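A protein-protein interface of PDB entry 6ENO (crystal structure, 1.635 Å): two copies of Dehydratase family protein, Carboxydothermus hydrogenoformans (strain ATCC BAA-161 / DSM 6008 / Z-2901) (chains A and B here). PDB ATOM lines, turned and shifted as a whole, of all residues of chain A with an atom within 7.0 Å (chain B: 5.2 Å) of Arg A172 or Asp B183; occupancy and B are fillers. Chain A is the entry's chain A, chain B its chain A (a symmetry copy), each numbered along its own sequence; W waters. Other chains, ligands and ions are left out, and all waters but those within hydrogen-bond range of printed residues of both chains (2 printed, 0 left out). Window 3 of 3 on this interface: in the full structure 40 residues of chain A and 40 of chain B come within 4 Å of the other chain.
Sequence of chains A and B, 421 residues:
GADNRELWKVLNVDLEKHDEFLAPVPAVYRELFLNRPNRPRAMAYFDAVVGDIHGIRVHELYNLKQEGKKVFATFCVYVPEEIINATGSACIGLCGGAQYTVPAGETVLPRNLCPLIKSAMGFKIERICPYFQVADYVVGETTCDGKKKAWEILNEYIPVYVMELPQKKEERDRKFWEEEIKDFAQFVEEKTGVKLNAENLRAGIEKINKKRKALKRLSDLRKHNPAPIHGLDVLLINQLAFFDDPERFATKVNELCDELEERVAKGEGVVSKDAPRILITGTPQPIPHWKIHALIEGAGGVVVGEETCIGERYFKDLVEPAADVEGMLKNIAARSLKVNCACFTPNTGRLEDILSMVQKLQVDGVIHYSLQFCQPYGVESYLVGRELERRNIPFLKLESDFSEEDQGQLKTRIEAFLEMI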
ATOM      1  N   PRO A 166     -13.823  23.186 -10.746  1.00  0.00           N
ATOM      2  CA  PRO A 166     -12.992  22.747  -9.606  1.00  0.00           C
ATOM      3  C   PRO A 166     -13.806  22.719  -8.321  1.00  0.00           C
ATOM      4  O   PRO A 166     -14.996  23.027  -8.337  1.00  0.00           O
ATOM      5  CB  PRO A 166     -11.884  23.802  -9.559  1.00  0.00           C
ATOM      6  CG  PRO A 166     -12.406  24.978 -10.194  1.00  0.00           C
ATOM      7  CD  PRO A 166     -13.442  24.550 -11.180  1.00  0.00           C
ATOM      8  N   LYS A 168     -12.393  23.940  -5.123  1.00  0.00           N
ATOM      9  CA  LYS A 168     -11.959  25.005  -4.231  1.00  0.00           C
ATOM     10  C   LYS A 168     -11.839  26.279  -5.063  1.00  0.00           C
ATOM     11  O   LYS A 168     -11.974  26.232  -6.290  1.00  0.00           O
ATOM     12  CB  LYS A 168     -10.594  24.693  -3.573  1.00  0.00           C
ATOM     13  CG  LYS A 168     -10.595  23.446  -2.689  1.00  0.00           C
ATOM     14  CD  LYS A 168      -9.259  23.311  -1.934  1.00  0.00           C
ATOM     15  CE  LYS A 168      -9.256  22.147  -0.971  1.00  0.00           C
ATOM     16  NZ  LYS A 168      -7.937  22.097  -0.238  1.00  0.00           N
ATOM     17  N   LYS A 169     -11.475  27.382  -4.415  1.00  0.00           N
ATOM     18  CA  LYS A 169     -11.293  28.668  -5.109  1.00  0.00           C
ATOM     19  C   LYS A 169      -9.915  29.259  -4.829  1.00  0.00           C
ATOM     20  O   LYS A 169      -9.738  30.487  -4.746  1.00  0.00           O
ATOM     21  CB  LYS A 169     -12.407  29.654  -4.743  1.00  0.00           C
ATOM     22  CG  LYS A 169     -13.815  29.166  -5.154  1.00  0.00           C
ATOM     23  CD  LYS A 169     -14.947  30.134  -4.835  1.00  0.00           C
ATOM     24  CE  LYS A 169     -16.275  29.726  -5.456  1.00  0.00           C
ATOM     25  NZ  LYS A 169     -17.312  30.758  -5.103  1.00  0.00           N
ATOM     26  N   GLU A 170      -8.909  28.394  -4.702  1.00  0.00           N
ATOM     27  CA  GLU A 170      -7.548  28.863  -4.577  1.00  0.00           C
ATOM     28  C   GLU A 170      -7.016  29.233  -5.959  1.00  0.00           C
ATOM     29  O   GLU A 170      -7.656  29.010  -6.985  1.00  0.00           O
ATOM     30  CB  GLU A 170      -6.691  27.807  -3.890  1.00  0.00           C
ATOM     31  CG  GLU A 170      -7.115  27.515  -2.443  1.00  0.00           C
ATOM     32  CD  GLU A 170      -6.721  28.616  -1.472  1.00  0.00           C
ATOM     33  OE1 GLU A 170      -5.959  29.520  -1.874  1.00  0.00           O
ATOM     34  OE2 GLU A 170      -7.167  28.587  -0.298  1.00  0.00           O
ATOM     35  N   GLU A 171      -5.831  29.830  -5.983  1.00  0.00           N
ATOM     36  CA  GLU A 171      -5.321  30.336  -7.251  1.00  0.00           C
ATOM     37  C   GLU A 171      -5.225  29.232  -8.310  1.00  0.00           C
ATOM     38  O   GLU A 171      -5.503  29.471  -9.482  1.00  0.00           O
ATOM     39  CB  GLU A 171      -3.972  31.005  -7.043  1.00  0.00           C
ATOM     40  CG  GLU A 171      -3.425  31.668  -8.314  1.00  0.00           C
ATOM     41  CD  GLU A 171      -4.167  32.946  -8.793  1.00  0.00           C
ATOM     42  OE1 GLU A 171      -5.256  33.336  -8.275  1.00  0.00           O
ATOM     43  OE2 GLU A 171      -3.620  33.578  -9.731  1.00  0.00           O
ATOM     44  N   ARG A 172      -4.845  28.024  -7.920  1.00  0.00           N
ATOM     45  CA  ARG A 172      -4.718  26.954  -8.903  1.00  0.00           C
ATOM     46  C   ARG A 172      -6.073  26.622  -9.514  1.00  0.00           C
ATOM     47  O   ARG A 172      -6.167  26.306 -10.709  1.00  0.00           O
ATOM     48  CB  ARG A 172      -4.091  25.723  -8.243  1.00  0.00           C
ATOM     49  CG  ARG A 172      -3.780  24.558  -9.169  1.00  0.00           C
ATOM     50  CD  ARG A 172      -2.986  23.453  -8.446  1.00  0.00           C
ATOM     51  NE  ARG A 172      -1.786  24.000  -7.820  1.00  0.00           N
ATOM     52  CZ  ARG A 172      -1.442  23.851  -6.541  1.00  0.00           C
ATOM     53  NH1 ARG A 172      -2.177  23.142  -5.695  1.00  0.00           N
ATOM     54  NH2 ARG A 172      -0.349  24.427  -6.108  1.00  0.00           N
ATOM     55  N   ASP A 173      -7.131  26.684  -8.698  1.00  0.00           N
ATOM     56  CA  ASP A 173      -8.486  26.446  -9.157  1.00  0.00           C
ATOM     57  C   ASP A 173      -8.933  27.519 -10.135  1.00  0.00           C
ATOM     58  O   ASP A 173      -9.599  27.229 -11.146  1.00  0.00           O
ATOM     59  CB  ASP A 173      -9.418  26.440  -7.949  1.00  0.00           C
ATOM     60  CG  ASP A 173      -9.064  25.362  -6.972  1.00  0.00           C
ATOM     61  OD1 ASP A 173      -9.352  24.185  -7.259  1.00  0.00           O
ATOM     62  OD2 ASP A 173      -8.485  25.694  -5.937  1.00  0.00           O
ATOM     63  N   ARG A 174      -8.612  28.771  -9.826  1.00  0.00           N
ATOM     64  CA  ARG A 174      -9.044  29.860 -10.695  1.00  0.00           C
ATOM     65  C   ARG A 174      -8.424  29.726 -12.070  1.00  0.00           C
ATOM     66  O   ARG A 174      -9.106  29.920 -13.071  1.00  0.00           O
ATOM     67  CB  ARG A 174      -8.700  31.209 -10.074  1.00  0.00           C
ATOM     68  CG  ARG A 174      -9.463  31.428  -8.758  1.00  0.00           C
ATOM     69  CD  ARG A 174      -9.159  32.751  -8.071  1.00  0.00           C
ATOM     70  NE  ARG A 174      -9.901  32.891  -6.811  1.00  0.00           N
ATOM     71  CZ  ARG A 174     -11.149  33.365  -6.708  1.00  0.00           C
ATOM     72  NH1 ARG A 174     -11.829  33.746  -7.788  1.00  0.00           N
ATOM     73  NH2 ARG A 174     -11.725  33.462  -5.515  1.00  0.00           N
ATOM     74  N   LYS A 175      -7.149  29.345 -12.135  1.00  0.00           N
ATOM     75  CA  LYS A 175      -6.502  29.172 -13.432  1.00  0.00           C
ATOM     76  C   LYS A 175      -7.055  27.954 -14.159  1.00  0.00           C
ATOM     77  O   LYS A 175      -7.246  27.972 -15.382  1.00  0.00           O
ATOM     78  CB  LYS A 175      -4.991  29.037 -13.250  1.00  0.00           C
ATOM     79  CG  LYS A 175      -4.239  28.911 -14.573  1.00  0.00           C
ATOM     80  CD  LYS A 175      -4.534  30.068 -15.521  1.00  0.00           C
ATOM     81  CE  LYS A 175      -4.108  29.750 -16.927  1.00  0.00           C
ATOM     82  NZ  LYS A 175      -2.638  29.668 -17.050  1.00  0.00           N
ATOM     83  N   PHE A 176      -7.317  26.888 -13.428  1.00  0.00           N
ATOM     84  CA  PHE A 176      -7.922  25.710 -14.019  1.00  0.00           C
ATOM     85  C   PHE A 176      -9.247  26.060 -14.694  1.00  0.00           C
ATOM     86  O   PHE A 176      -9.511  25.682 -15.844  1.00  0.00           O
ATOM     87  CB  PHE A 176      -8.098  24.691 -12.899  1.00  0.00           C
ATOM     88  CG  PHE A 176      -8.570  23.364 -13.355  1.00  0.00           C
ATOM     89  CD1 PHE A 176      -9.949  23.129 -13.561  1.00  0.00           C
ATOM     90  CD2 PHE A 176      -7.664  22.350 -13.573  1.00  0.00           C
ATOM     91  CE1 PHE A 176     -10.402  21.879 -13.961  1.00  0.00           C
ATOM     92  CE2 PHE A 176      -8.120  21.066 -13.967  1.00  0.00           C
ATOM     93  CZ  PHE A 176      -9.489  20.856 -14.184  1.00  0.00           C
ATOM     94  N   TRP A 177     -10.071  26.833 -14.000  1.00  0.00           N
ATOM     95  CA  TRP A 177     -11.404  27.154 -14.507  1.00  0.00           C
ATOM     96  C   TRP A 177     -11.309  28.085 -15.703  1.00  0.00           C
ATOM     97  O   TRP A 177     -12.065  27.937 -16.666  1.00  0.00           O
ATOM     98  CB  TRP A 177     -12.233  27.753 -13.381  1.00  0.00           C
ATOM     99  CG  TRP A 177     -13.602  28.143 -13.772  1.00  0.00           C
ATOM    100  CD1 TRP A 177     -14.149  29.408 -13.698  1.00  0.00           C
ATOM    101  CD2 TRP A 177     -14.626  27.295 -14.294  1.00  0.00           C
ATOM    102  NE1 TRP A 177     -15.466  29.374 -14.129  1.00  0.00           N
ATOM    103  CE2 TRP A 177     -15.773  28.100 -14.506  1.00  0.00           C
ATOM    104  CE3 TRP A 177     -14.695  25.933 -14.589  1.00  0.00           C
ATOM    105  CZ2 TRP A 177     -16.951  27.585 -15.006  1.00  0.00           C
ATOM    106  CZ3 TRP A 177     -15.873  25.430 -15.094  1.00  0.00           C
ATOM    107  CH2 TRP A 177     -16.977  26.264 -15.303  1.00  0.00           C
ATOM    108  N   TYR B 161      -6.584  18.359   6.844  1.00  0.00           N
ATOM    109  CA  TYR B 161      -5.955  18.859   5.625  1.00  0.00           C
ATOM    110  C   TYR B 161      -6.746  18.320   4.453  1.00  0.00           C
ATOM    111  O   TYR B 161      -6.862  17.104   4.309  1.00  0.00           O
ATOM    112  CB  TYR B 161      -4.507  18.385   5.538  1.00  0.00           C
ATOM    113  CG  TYR B 161      -3.796  18.886   4.300  1.00  0.00           C
ATOM    114  CD1 TYR B 161      -3.955  18.237   3.095  1.00  0.00           C
ATOM    115  CD2 TYR B 161      -3.001  20.004   4.350  1.00  0.00           C
ATOM    116  CE1 TYR B 161      -3.330  18.684   1.950  1.00  0.00           C
ATOM    117  CE2 TYR B 161      -2.347  20.469   3.224  1.00  0.00           C
ATOM    118  CZ  TYR B 161      -2.540  19.814   2.013  1.00  0.00           C
ATOM    119  OH  TYR B 161      -1.934  20.294   0.884  1.00  0.00           O
ATOM    120  N   PHE B 176      -2.586  19.072 -12.294  1.00  0.00           N
ATOM    121  CA  PHE B 176      -3.200  19.602 -11.092  1.00  0.00           C
ATOM    122  C   PHE B 176      -2.917  18.697  -9.893  1.00  0.00           C
ATOM    123  O   PHE B 176      -2.507  19.153  -8.816  1.00  0.00           O
ATOM    124  CB  PHE B 176      -4.693  19.732 -11.374  1.00  0.00           C
ATOM    125  CG  PHE B 176      -5.457  20.401 -10.298  1.00  0.00           C
ATOM    126  CD1 PHE B 176      -5.904  19.664  -9.176  1.00  0.00           C
ATOM    127  CD2 PHE B 176      -5.744  21.745 -10.390  1.00  0.00           C
ATOM    128  CE1 PHE B 176      -6.645  20.277  -8.176  1.00  0.00           C
ATOM    129  CE2 PHE B 176      -6.515  22.376  -9.380  1.00  0.00           C
ATOM    130  CZ  PHE B 176      -6.933  21.634  -8.267  1.00  0.00           C
ATOM    131  N   GLU B 179       0.525  18.874  -8.531  1.00  0.00           N
ATOM    132  CA  GLU B 179       0.767  20.025  -7.665  1.00  0.00           C
ATOM    133  C   GLU B 179       0.153  19.817  -6.288  1.00  0.00           C
ATOM    134  O   GLU B 179       0.717  20.253  -5.281  1.00  0.00           O
ATOM    135  CB  GLU B 179       0.224  21.301  -8.288  1.00  0.00           C
ATOM    136  CG  GLU B 179       0.931  21.723  -9.598  1.00  0.00           C
ATOM    137  CD  GLU B 179       2.434  21.877  -9.411  1.00  0.00           C
ATOM    138  OE1 GLU B 179       2.848  22.485  -8.394  1.00  0.00           O
ATOM    139  OE2 GLU B 179       3.202  21.378 -10.261  1.00  0.00           O
ATOM    140  N   GLU B 180      -1.018  19.162  -6.228  1.00  0.00           N
ATOM    141  CA  GLU B 180      -1.644  18.840  -4.949  1.00  0.00           C
ATOM    142  C   GLU B 180      -0.735  17.945  -4.111  1.00  0.00           C
ATOM    143  O   GLU B 180      -0.605  18.116  -2.891  1.00  0.00           O
ATOM    144  CB  GLU B 180      -2.987  18.146  -5.169  1.00  0.00           C
ATOM    145  CG  GLU B 180      -4.084  19.086  -5.524  1.00  0.00           C
ATOM    146  CD  GLU B 180      -4.492  19.993  -4.362  1.00  0.00           C
ATOM    147  OE1 GLU B 180      -4.623  19.496  -3.193  1.00  0.00           O
ATOM    148  OE2 GLU B 180      -4.657  21.187  -4.630  1.00  0.00           O
ATOM    149  N   ILE B 181      -0.114  16.960  -4.748  1.00  0.00           N
ATOM    150  CA  ILE B 181       0.809  16.065  -4.049  1.00  0.00           C
ATOM    151  C   ILE B 181       2.028  16.828  -3.536  1.00  0.00           C
ATOM    152  O   ILE B 181       2.496  16.588  -2.412  1.00  0.00           O
ATOM    153  CB  ILE B 181       1.199  14.914  -4.990  1.00  0.00           C
ATOM    154  CG1 ILE B 181      -0.026  14.003  -5.176  1.00  0.00           C
ATOM    155  CG2 ILE B 181       2.413  14.167  -4.521  1.00  0.00           C
ATOM    156  CD1 ILE B 181      -0.420  13.222  -3.995  1.00  0.00           C
ATOM    157  N   LYS B 182       2.531  17.784  -4.309  1.00  0.00           N
ATOM    158  CA  LYS B 182       3.636  18.621  -3.844  1.00  0.00           C
ATOM    159  C   LYS B 182       3.242  19.449  -2.623  1.00  0.00           C
ATOM    160  O   LYS B 182       4.025  19.570  -1.670  1.00  0.00           O
ATOM    161  CB  LYS B 182       4.142  19.515  -4.980  1.00  0.00           C
ATOM    162  CG  LYS B 182       4.991  18.733  -5.961  1.00  0.00           C
ATOM    163  CD  LYS B 182       4.902  19.276  -7.369  1.00  0.00           C
ATOM    164  CE  LYS B 182       5.589  20.615  -7.515  1.00  0.00           C
ATOM    165  NZ  LYS B 182       5.696  21.020  -8.973  1.00  0.00           N
ATOM    166  N   ASP B 183       2.044  20.055  -2.644  1.00  0.00           N
ATOM    167  CA  ASP B 183       1.602  20.838  -1.507  1.00  0.00           C
ATOM    168  C   ASP B 183       1.410  19.950  -0.292  1.00  0.00           C
ATOM    169  O   ASP B 183       1.767  20.337   0.829  1.00  0.00           O
ATOM    170  CB  ASP B 183       0.299  21.588  -1.810  1.00  0.00           C
ATOM    171  CG  ASP B 183       0.478  22.752  -2.786  1.00  0.00           C
ATOM    172  OD1 ASP B 183       1.615  23.111  -3.147  1.00  0.00           O
ATOM    173  OD2 ASP B 183      -0.564  23.315  -3.194  1.00  0.00           O
ATOM    174  N   PHE B 184       0.899  18.732  -0.499  1.00  0.00           N
ATOM    175  CA  PHE B 184       0.751  17.815   0.629  1.00  0.00           C
ATOM    176  C   PHE B 184       2.117  17.430   1.204  1.00  0.00           C
ATOM    177  O   PHE B 184       2.293  17.404   2.427  1.00  0.00           O
ATOM    178  CB  PHE B 184      -0.042  16.577   0.188  1.00  0.00           C
ATOM    179  CG  PHE B 184      -0.207  15.533   1.273  1.00  0.00           C
ATOM    180  CD1 PHE B 184      -0.989  15.796   2.374  1.00  0.00           C
ATOM    181  CD2 PHE B 184       0.455  14.322   1.190  1.00  0.00           C
ATOM    182  CE1 PHE B 184      -1.143  14.872   3.365  1.00  0.00           C
ATOM    183  CE2 PHE B 184       0.305  13.397   2.191  1.00  0.00           C
ATOM    184  CZ  PHE B 184      -0.503  13.680   3.286  1.00  0.00           C
ATOM    185  N   ALA B 185       3.096  17.150   0.338  1.00  0.00           N
ATOM    186  CA  ALA B 185       4.441  16.825   0.808  1.00  0.00           C
ATOM    187  C   ALA B 185       4.976  17.931   1.706  1.00  0.00           C
ATOM    188  O   ALA B 185       5.568  17.654   2.758  1.00  0.00           O
ATOM    189  CB  ALA B 185       5.383  16.591  -0.381  1.00  0.00           C
ATOM    190  N   GLN B 186       4.776  19.190   1.316  1.00  0.00           N
ATOM    191  CA  GLN B 186       5.269  20.302   2.131  1.00  0.00           C
ATOM    192  C   GLN B 186       4.585  20.336   3.490  1.00  0.00           C
ATOM    193  O   GLN B 186       5.220  20.661   4.498  1.00  0.00           O
ATOM    194  CB  GLN B 186       5.060  21.635   1.417  1.00  0.00           C
ATOM    195  CG  GLN B 186       6.133  21.980   0.417  1.00  0.00           C
ATOM    196  CD  GLN B 186       5.975  23.381  -0.157  1.00  0.00           C
ATOM    197  OE1 GLN B 186       5.246  24.228   0.386  1.00  0.00           O
ATOM    198  NE2 GLN B 186       6.654  23.628  -1.263  1.00  0.00           N
ATOM    199  N   PHE B 187       3.278  20.058   3.523  1.00  0.00           N
ATOM    200  CA  PHE B 187       2.550  19.970   4.793  1.00  0.00           C
ATOM    201  C   PHE B 187       3.118  18.847   5.652  1.00  0.00           C
ATOM    202  O   PHE B 187       3.395  19.033   6.845  1.00  0.00           O
ATOM    203  CB  PHE B 187       1.044  19.772   4.513  1.00  0.00           C
ATOM    204  CG  PHE B 187       0.194  19.337   5.717  1.00  0.00           C
ATOM    205  CD1 PHE B 187      -0.255  20.253   6.654  1.00  0.00           C
ATOM    206  CD2 PHE B 187      -0.216  18.017   5.829  1.00  0.00           C
ATOM    207  CE1 PHE B 187      -1.068  19.842   7.717  1.00  0.00           C
ATOM    208  CE2 PHE B 187      -1.007  17.597   6.883  1.00  0.00           C
ATOM    209  CZ  PHE B 187      -1.435  18.532   7.829  1.00  0.00           C
HETATM  210  O   HOH W   1      -6.360  23.974  -4.940  1.00  0.00           O
HETATM  211  O   HOH W   2       1.964  25.608  -4.469  1.00  0.00           O
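Of the printed residues of chain B, Arg A172 touches Phe B176 (3.5 Å), Glu B179 (3.4 Å), Glu B180 (3.3 Å) and Asp B183 (3.0 Å). Of the printed residues of chain A, Glu B179 touches Arg A172 (3.4 Å). Printed residues of chain A within 4 Å of Glu B180: Arg A172. Printed residues of chain A within 4 Å of Asp B183: Arg A172 (3.0 Å). Ala B185 touches none of the printed residues of chain A. The nearest printed residue of chain B that does not touch Arg A172 is Ile B181 (6.6 Å). The nearest printed residue of chain A that does not touch Asp B183 is Glu A170 (7.6 Å). The nearest printed residue of chain A that does not touch Glu B180 is Lys A168 (5.1 Å).
OD2 of Asp A173 lies within hydrogen-bond range of N of Glu A170 (3.0 Å). The side-chain amino group (NZ) of Lys B182 is in salt-bridge range of the side-chain carboxylate (OE2) of Glu B179, at 2.8 Å.
Phe B176 touches Arg A172 (CE2 to CG, 3.5 Å). Arg A172 touches Glu B179. OD1 of Asp A173 touches CZ of Phe B176, 3.7 Å away. Phe A176 touches Phe B176 (CD2 to CD2, 3.8 Å).
Water W2 bridges OD1 of Asp B183 (2.8 Å) and NH2 of Arg A172 (3.1 Å). Water W1 lies within hydrogen-bond range of OD2 of Asp A173 (2.9 Å) and OE2 of Glu B180 (3.3 Å).
OE2 of Glu B180 lies within salt-bridge range of NH1 of Arg A172, 3.3 Å away. The guanidinium group (NH1) of Arg A172 lies within salt-bridge range of the side-chain carboxylate (OD2) of Asp B183 (3.0 Å).
Hydrophobic or aromatic side chains of chain A that line the printed part of chain B: Phe A176. Along chain A the printed residues that touch a printed residue of chain B span positions 172 to 176. Hydrophobic or aromatic side chains of chain B that line the printed part of chain A: Phe B176. Among the printed residues, 6 pairs touch across the chains. Among the printed residues, Asp or Glu carboxylates within 4 Å of a Lys or Arg side-chain nitrogen of the other chain: Arg A172 with Glu B180 and Arg A172 with Asp B183.
Phe B176 touches its own counterpart, Phe A176. Position printed for both chains: 176. Of the 6 pairs that touch across the chains among the printed residues, 1 has its exchanged pair printed and touching as well.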
